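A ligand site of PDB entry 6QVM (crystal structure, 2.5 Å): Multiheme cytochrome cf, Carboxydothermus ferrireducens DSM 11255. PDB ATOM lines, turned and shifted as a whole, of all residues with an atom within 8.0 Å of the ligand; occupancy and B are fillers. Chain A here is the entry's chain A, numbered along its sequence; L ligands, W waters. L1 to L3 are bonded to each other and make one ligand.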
ATOM      1  N   ASN A 398      -1.015  28.849 -24.650  1.00  0.00           N
ATOM      2  CA  ASN A 398      -0.316  27.776 -25.343  1.00  0.00           C
ATOM      3  C   ASN A 398      -0.595  26.413 -24.729  1.00  0.00           C
ATOM      4  O   ASN A 398       0.189  25.471 -24.919  1.00  0.00           O
ATOM      5  CB  ASN A 398       1.193  28.040 -25.381  1.00  0.00           C
ATOM      6  CG  ASN A 398       1.815  28.142 -23.998  1.00  0.00           C
ATOM      7  OD1 ASN A 398       1.166  27.926 -22.979  1.00  0.00           O
ATOM      8  ND2 ASN A 398       3.101  28.473 -23.955  1.00  0.00           N
ATOM      9  N   ASP A 399      -1.686  26.280 -23.985  1.00  0.00           N
ATOM     10  CA  ASP A 399      -1.987  25.049 -23.273  1.00  0.00           C
ATOM     11  C   ASP A 399      -2.748  24.082 -24.172  1.00  0.00           C
ATOM     12  O   ASP A 399      -3.074  24.372 -25.328  1.00  0.00           O
ATOM     13  CB  ASP A 399      -2.781  25.362 -22.001  1.00  0.00           C
ATOM     14  CG  ASP A 399      -1.914  25.918 -20.892  1.00  0.00           C
ATOM     15  OD1 ASP A 399      -0.688  26.063 -21.118  1.00  0.00           O
ATOM     16  OD2 ASP A 399      -2.449  26.200 -19.793  1.00  0.00           O
ATOM     17  N   GLU A 400      -3.055  22.905 -23.625  1.00  0.00           N
ATOM     18  CA  GLU A 400      -3.832  21.879 -24.293  1.00  0.00           C
ATOM     19  C   GLU A 400      -5.257  21.897 -23.741  1.00  0.00           C
ATOM     20  O   GLU A 400      -5.454  21.827 -22.527  1.00  0.00           O
ATOM     21  CB  GLU A 400      -3.196  20.506 -24.080  1.00  0.00           C
ATOM     22  CG  GLU A 400      -3.927  19.343 -24.720  1.00  0.00           C
ATOM     23  CD  GLU A 400      -3.231  18.008 -24.465  1.00  0.00           C
ATOM     24  OE1 GLU A 400      -3.511  17.036 -25.191  1.00  0.00           O
ATOM     25  OE2 GLU A 400      -2.393  17.960 -23.531  1.00  0.00           O
ATOM     26  N   TYR A 401      -6.240  21.992 -24.640  1.00  0.00           N
ATOM     27  CA  TYR A 401      -7.633  22.198 -24.253  1.00  0.00           C
ATOM     28  C   TYR A 401      -8.472  20.976 -24.583  1.00  0.00           C
ATOM     29  O   TYR A 401      -8.340  20.385 -25.652  1.00  0.00           O
ATOM     30  CB  TYR A 401      -8.250  23.396 -24.985  1.00  0.00           C
ATOM     31  CG  TYR A 401      -7.406  24.635 -25.098  1.00  0.00           C
ATOM     32  CD1 TYR A 401      -6.537  25.017 -24.077  1.00  0.00           C
ATOM     33  CD2 TYR A 401      -7.492  25.443 -26.226  1.00  0.00           C
ATOM     34  CE1 TYR A 401      -5.769  26.157 -24.188  1.00  0.00           C
ATOM     35  CE2 TYR A 401      -6.730  26.580 -26.344  1.00  0.00           C
ATOM     36  CZ  TYR A 401      -5.877  26.936 -25.324  1.00  0.00           C
ATOM     37  OH  TYR A 401      -5.117  28.075 -25.456  1.00  0.00           O
ATOM     38  N   ALA A 402      -9.372  20.635 -23.662  1.00  0.00           N
ATOM     39  CA  ALA A 402     -10.505  19.765 -23.946  1.00  0.00           C
ATOM     40  C   ALA A 402     -11.737  20.659 -23.917  1.00  0.00           C
ATOM     41  O   ALA A 402     -12.255  20.999 -22.848  1.00  0.00           O
ATOM     42  CB  ALA A 402     -10.608  18.625 -22.927  1.00  0.00           C
ATOM     43  N   GLY A 408     -11.655  14.917 -28.809  1.00  0.00           N
ATOM     44  CA  GLY A 408     -10.270  15.271 -29.067  1.00  0.00           C
ATOM     45  C   GLY A 408      -9.808  16.401 -28.167  1.00  0.00           C
ATOM     46  O   GLY A 408     -10.565  16.988 -27.394  1.00  0.00           O
ATOM     47  N   THR A 409      -8.510  16.706 -28.265  1.00  0.00           N
ATOM     48  CA  THR A 409      -7.955  17.866 -27.593  1.00  0.00           C
ATOM     49  C   THR A 409      -7.135  18.676 -28.589  1.00  0.00           C
ATOM     50  O   THR A 409      -6.754  18.190 -29.663  1.00  0.00           O
ATOM     51  CB  THR A 409      -7.074  17.476 -26.398  1.00  0.00           C
ATOM     52  OG1 THR A 409      -5.899  16.803 -26.844  1.00  0.00           O
ATOM     53  CG2 THR A 409      -7.846  16.593 -25.423  1.00  0.00           C
ATOM     54  N   VAL A 410      -6.889  19.943 -28.238  1.00  0.00           N
ATOM     55  CA  VAL A 410      -6.291  20.887 -29.174  1.00  0.00           C
ATOM     56  C   VAL A 410      -5.358  21.806 -28.391  1.00  0.00           C
ATOM     57  O   VAL A 410      -5.584  22.095 -27.214  1.00  0.00           O
ATOM     58  CB  VAL A 410      -7.391  21.694 -29.907  1.00  0.00           C
ATOM     59  CG1 VAL A 410      -7.640  23.019 -29.227  1.00  0.00           C
ATOM     60  CG2 VAL A 410      -7.050  21.877 -31.379  1.00  0.00           C
ATOM     61  N   TYR A 411      -4.286  22.227 -29.046  1.00  0.00           N
ATOM     62  CA  TYR A 411      -3.339  23.173 -28.462  1.00  0.00           C
ATOM     63  C   TYR A 411      -3.705  24.591 -28.868  1.00  0.00           C
ATOM     64  O   TYR A 411      -4.042  24.837 -30.035  1.00  0.00           O
ATOM     65  CB  TYR A 411      -1.898  22.860 -28.896  1.00  0.00           C
ATOM     66  CG  TYR A 411      -1.306  21.568 -28.367  1.00  0.00           C
ATOM     67  CD1 TYR A 411      -0.876  21.455 -27.049  1.00  0.00           C
ATOM     68  CD2 TYR A 411      -1.163  20.458 -29.188  1.00  0.00           C
ATOM     69  CE1 TYR A 411      -0.330  20.278 -26.565  1.00  0.00           C
ATOM     70  CE2 TYR A 411      -0.619  19.272 -28.727  1.00  0.00           C
ATOM     71  CZ  TYR A 411      -0.202  19.187 -27.411  1.00  0.00           C
ATOM     72  OH  TYR A 411       0.337  18.020 -26.940  1.00  0.00           O
ATOM     73  N   ASP A 571     -11.568  22.426 -20.336  1.00  0.00           N
ATOM     74  CA  ASP A 571     -10.693  21.781 -19.367  1.00  0.00           C
ATOM     75  C   ASP A 571      -9.265  21.920 -19.857  1.00  0.00           C
ATOM     76  O   ASP A 571      -8.906  21.404 -20.925  1.00  0.00           O
ATOM     77  CB  ASP A 571     -11.068  20.311 -19.158  1.00  0.00           C
ATOM     78  CG  ASP A 571     -12.295  20.146 -18.276  1.00  0.00           C
ATOM     79  OD1 ASP A 571     -12.957  21.161 -17.973  1.00  0.00           O
ATOM     80  OD2 ASP A 571     -12.594  18.992 -17.876  1.00  0.00           O
ATOM     81  N   ASN A 572      -8.451  22.646 -19.087  1.00  0.00           N
ATOM     82  CA  ASN A 572      -7.049  22.887 -19.418  1.00  0.00           C
ATOM     83  C   ASN A 572      -6.247  21.693 -18.941  1.00  0.00           C
ATOM     84  O   ASN A 572      -5.944  21.559 -17.756  1.00  0.00           O
ATOM     85  CB  ASN A 572      -6.581  24.192 -18.783  1.00  0.00           C
ATOM     86  CG  ASN A 572      -5.281  24.688 -19.366  1.00  0.00           C
ATOM     87  OD1 ASN A 572      -4.390  23.897 -19.698  1.00  0.00           O
ATOM     88  ND2 ASN A 572      -5.152  26.002 -19.506  1.00  0.00           N
ATOM     89  N   LEU A 573      -5.895  20.809 -19.876  1.00  0.00           N
ATOM     90  CA  LEU A 573      -5.161  19.599 -19.515  1.00  0.00           C
ATOM     91  C   LEU A 573      -3.710  19.880 -19.166  1.00  0.00           C
ATOM     92  O   LEU A 573      -3.089  19.077 -18.463  1.00  0.00           O
ATOM     93  CB  LEU A 573      -5.238  18.574 -20.655  1.00  0.00           C
ATOM     94  CG  LEU A 573      -6.670  18.131 -20.955  1.00  0.00           C
ATOM     95  CD1 LEU A 573      -6.726  17.091 -22.062  1.00  0.00           C
ATOM     96  CD2 LEU A 573      -7.318  17.594 -19.690  1.00  0.00           C
ATOM     97  N   THR A 574      -3.153  21.003 -19.623  1.00  0.00           N
ATOM     98  CA  THR A 574      -1.817  21.397 -19.198  1.00  0.00           C
ATOM     99  C   THR A 574      -1.799  21.751 -17.715  1.00  0.00           C
ATOM    100  O   THR A 574      -0.889  21.349 -16.983  1.00  0.00           O
ATOM    101  CB  THR A 574      -1.309  22.571 -20.024  1.00  0.00           C
ATOM    102  OG1 THR A 574      -1.452  22.283 -21.428  1.00  0.00           O
ATOM    103  CG2 THR A 574       0.156  22.834 -19.721  1.00  0.00           C
ATOM    104  N   LYS A 576      -4.106  20.638 -15.592  1.00  0.00           N
ATOM    105  CA  LYS A 576      -4.582  19.481 -14.846  1.00  0.00           C
ATOM    106  C   LYS A 576      -3.482  18.469 -14.554  1.00  0.00           C
ATOM    107  O   LYS A 576      -3.511  17.807 -13.511  1.00  0.00           O
ATOM    108  CB  LYS A 576      -5.731  18.815 -15.618  1.00  0.00           C
ATOM    109  CG  LYS A 576      -6.411  17.688 -14.863  1.00  0.00           C
ATOM    110  CD  LYS A 576      -7.442  16.996 -15.743  1.00  0.00           C
ATOM    111  CE  LYS A 576      -8.110  15.843 -14.999  1.00  0.00           C
ATOM    112  NZ  LYS A 576      -9.269  15.293 -15.748  1.00  0.00           N
ATOM    113  N   ASN A 577      -2.496  18.345 -15.449  1.00  0.00           N
ATOM    114  CA  ASN A 577      -1.482  17.305 -15.353  1.00  0.00           C
ATOM    115  C   ASN A 577      -0.116  17.855 -14.947  1.00  0.00           C
ATOM    116  O   ASN A 577       0.915  17.320 -15.361  1.00  0.00           O
ATOM    117  CB  ASN A 577      -1.375  16.539 -16.671  1.00  0.00           C
ATOM    118  CG  ASN A 577      -2.692  15.926 -17.090  1.00  0.00           C
ATOM    119  OD1 ASN A 577      -3.096  16.040 -18.246  1.00  0.00           O
ATOM    120  ND2 ASN A 577      -3.382  15.282 -16.151  1.00  0.00           N
HETATM  121  C1  LIG L   1       0.153  17.407 -25.724  1.00  0.00           C
HETATM  122  C2  LIG L   1       0.083  15.892 -25.508  1.00  0.00           C
HETATM  123  C3  LIG L   1       0.206  15.553 -24.016  1.00  0.00           C
HETATM  124  C4  LIG L   1       1.458  16.248 -23.494  1.00  0.00           C
HETATM  125  C5  LIG L   1       1.484  17.738 -23.817  1.00  0.00           C
HETATM  126  C6  LIG L   1       2.791  18.387 -23.363  1.00  0.00           C
HETATM  127  C7  LIG L   1      -1.156  15.020 -27.444  1.00  0.00           C
HETATM  128  C8  LIG L   1       0.149  14.891 -28.163  1.00  0.00           C
HETATM  129  N1  LIG L   1      -1.138  15.456 -26.172  1.00  0.00           N
HETATM  130  O1  LIG L   1       0.296  14.155 -23.701  1.00  0.00           O
HETATM  131  O2  LIG L   1       2.584  15.661 -24.111  1.00  0.00           O
HETATM  132  O3  LIG L   1       1.350  17.943 -25.203  1.00  0.00           O
HETATM  133  O4  LIG L   1       2.832  18.427 -21.958  1.00  0.00           O
HETATM  134  O5  LIG L   1      -2.204  14.717 -28.029  1.00  0.00           O
HETATM  135  C1  LG2 L   2      -1.023  13.546 -23.891  1.00  0.00           C
HETATM  136  C2  LG2 L   2      -1.018  11.993 -23.895  1.00  0.00           C
HETATM  137  C3  LG2 L   2      -2.355  11.783 -24.597  1.00  0.00           C
HETATM  138  C4  LG2 L   2      -3.475  12.352 -23.747  1.00  0.00           C
HETATM  139  C5  LG2 L   2      -3.223  13.795 -23.417  1.00  0.00           C
HETATM  140  C6  LG2 L   2      -4.297  14.316 -22.471  1.00  0.00           C
HETATM  141  C7  LG2 L   2       1.094  10.617 -23.987  1.00  0.00           C
HETATM  142  C8  LG2 L   2       2.392  10.476 -24.736  1.00  0.00           C
HETATM  143  N1  LG2 L   2       0.178  11.465 -24.532  1.00  0.00           N
HETATM  144  O1  LG2 L   2      -2.914  10.514 -24.753  1.00  0.00           O
HETATM  145  O2  LG2 L   2      -3.544  11.592 -22.562  1.00  0.00           O
HETATM  146  O3  LG2 L   2      -1.928  13.909 -22.845  1.00  0.00           O
HETATM  147  O4  LG2 L   2      -4.030  15.693 -22.323  1.00  0.00           O
HETATM  148  O5  LG2 L   2       0.931   9.955 -22.951  1.00  0.00           O
HETATM  149  C1  LG3 L   3      -2.061   9.576 -25.394  1.00  0.00           C
HETATM  150  C2  LG3 L   3      -2.902   8.403 -25.903  1.00  0.00           C
HETATM  151  C3  LG3 L   3      -1.822   7.473 -25.334  1.00  0.00           C
HETATM  152  C4  LG3 L   3      -0.452   7.754 -26.044  1.00  0.00           C
HETATM  153  C5  LG3 L   3      -0.268   9.180 -26.705  1.00  0.00           C
HETATM  154  C6  LG3 L   3       0.274   9.061 -28.135  1.00  0.00           C
HETATM  155  C7  LG3 L   3      -5.366   8.346 -26.073  1.00  0.00           C
HETATM  156  C8  LG3 L   3      -6.034   9.645 -26.364  1.00  0.00           C
HETATM  157  N1  LG3 L   3      -4.249   8.377 -25.342  1.00  0.00           N
HETATM  158  O1  LG3 L   3      -2.193   6.101 -25.335  1.00  0.00           O
HETATM  159  O2  LG3 L   3      -0.169   6.728 -26.990  1.00  0.00           O
HETATM  160  O3  LG3 L   3      -1.438  10.018 -26.603  1.00  0.00           O
HETATM  161  O4  LG3 L   3      -0.195  10.129 -28.919  1.00  0.00           O
HETATM  162  O5  LG3 L   3      -5.881   7.330 -26.480  1.00  0.00           O
HETATM  163  O   HOH W   1      -0.489  19.738 -22.098  1.00  0.00           O
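O of Glu 400 sits at hydrogen-bond distance from N of Leu 573 (2.9 Å).
The side-chain carboxylate (OE1) of Glu 400 sits at hydrogen-bond distance from the side-chain hydroxyl (OG1) of Thr 409 (2.9 Å).
The side-chain hydroxyl (OG1) of Thr 574 sits at hydrogen-bond distance from the backbone NH (N) of Glu 400 (2.8 Å).
O of Leu 573 sits close to OD1 of Asn 577.
OH of Tyr 411 is covalently linked to C1 of LIG L1 (1.4 Å).
The side-chain carboxylate (OE1) of Glu 400 is in hydrogen-bond range of a nitrogen (N1) of LIG L1 (3.0 Å).
CD1 of Leu 573 touches O4 of LG2 L2, 3.0 Å away.
Water W1 bridges OG1 of Thr 574 (2.8 Å) and OE2 of Glu 400 (3.0 Å).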
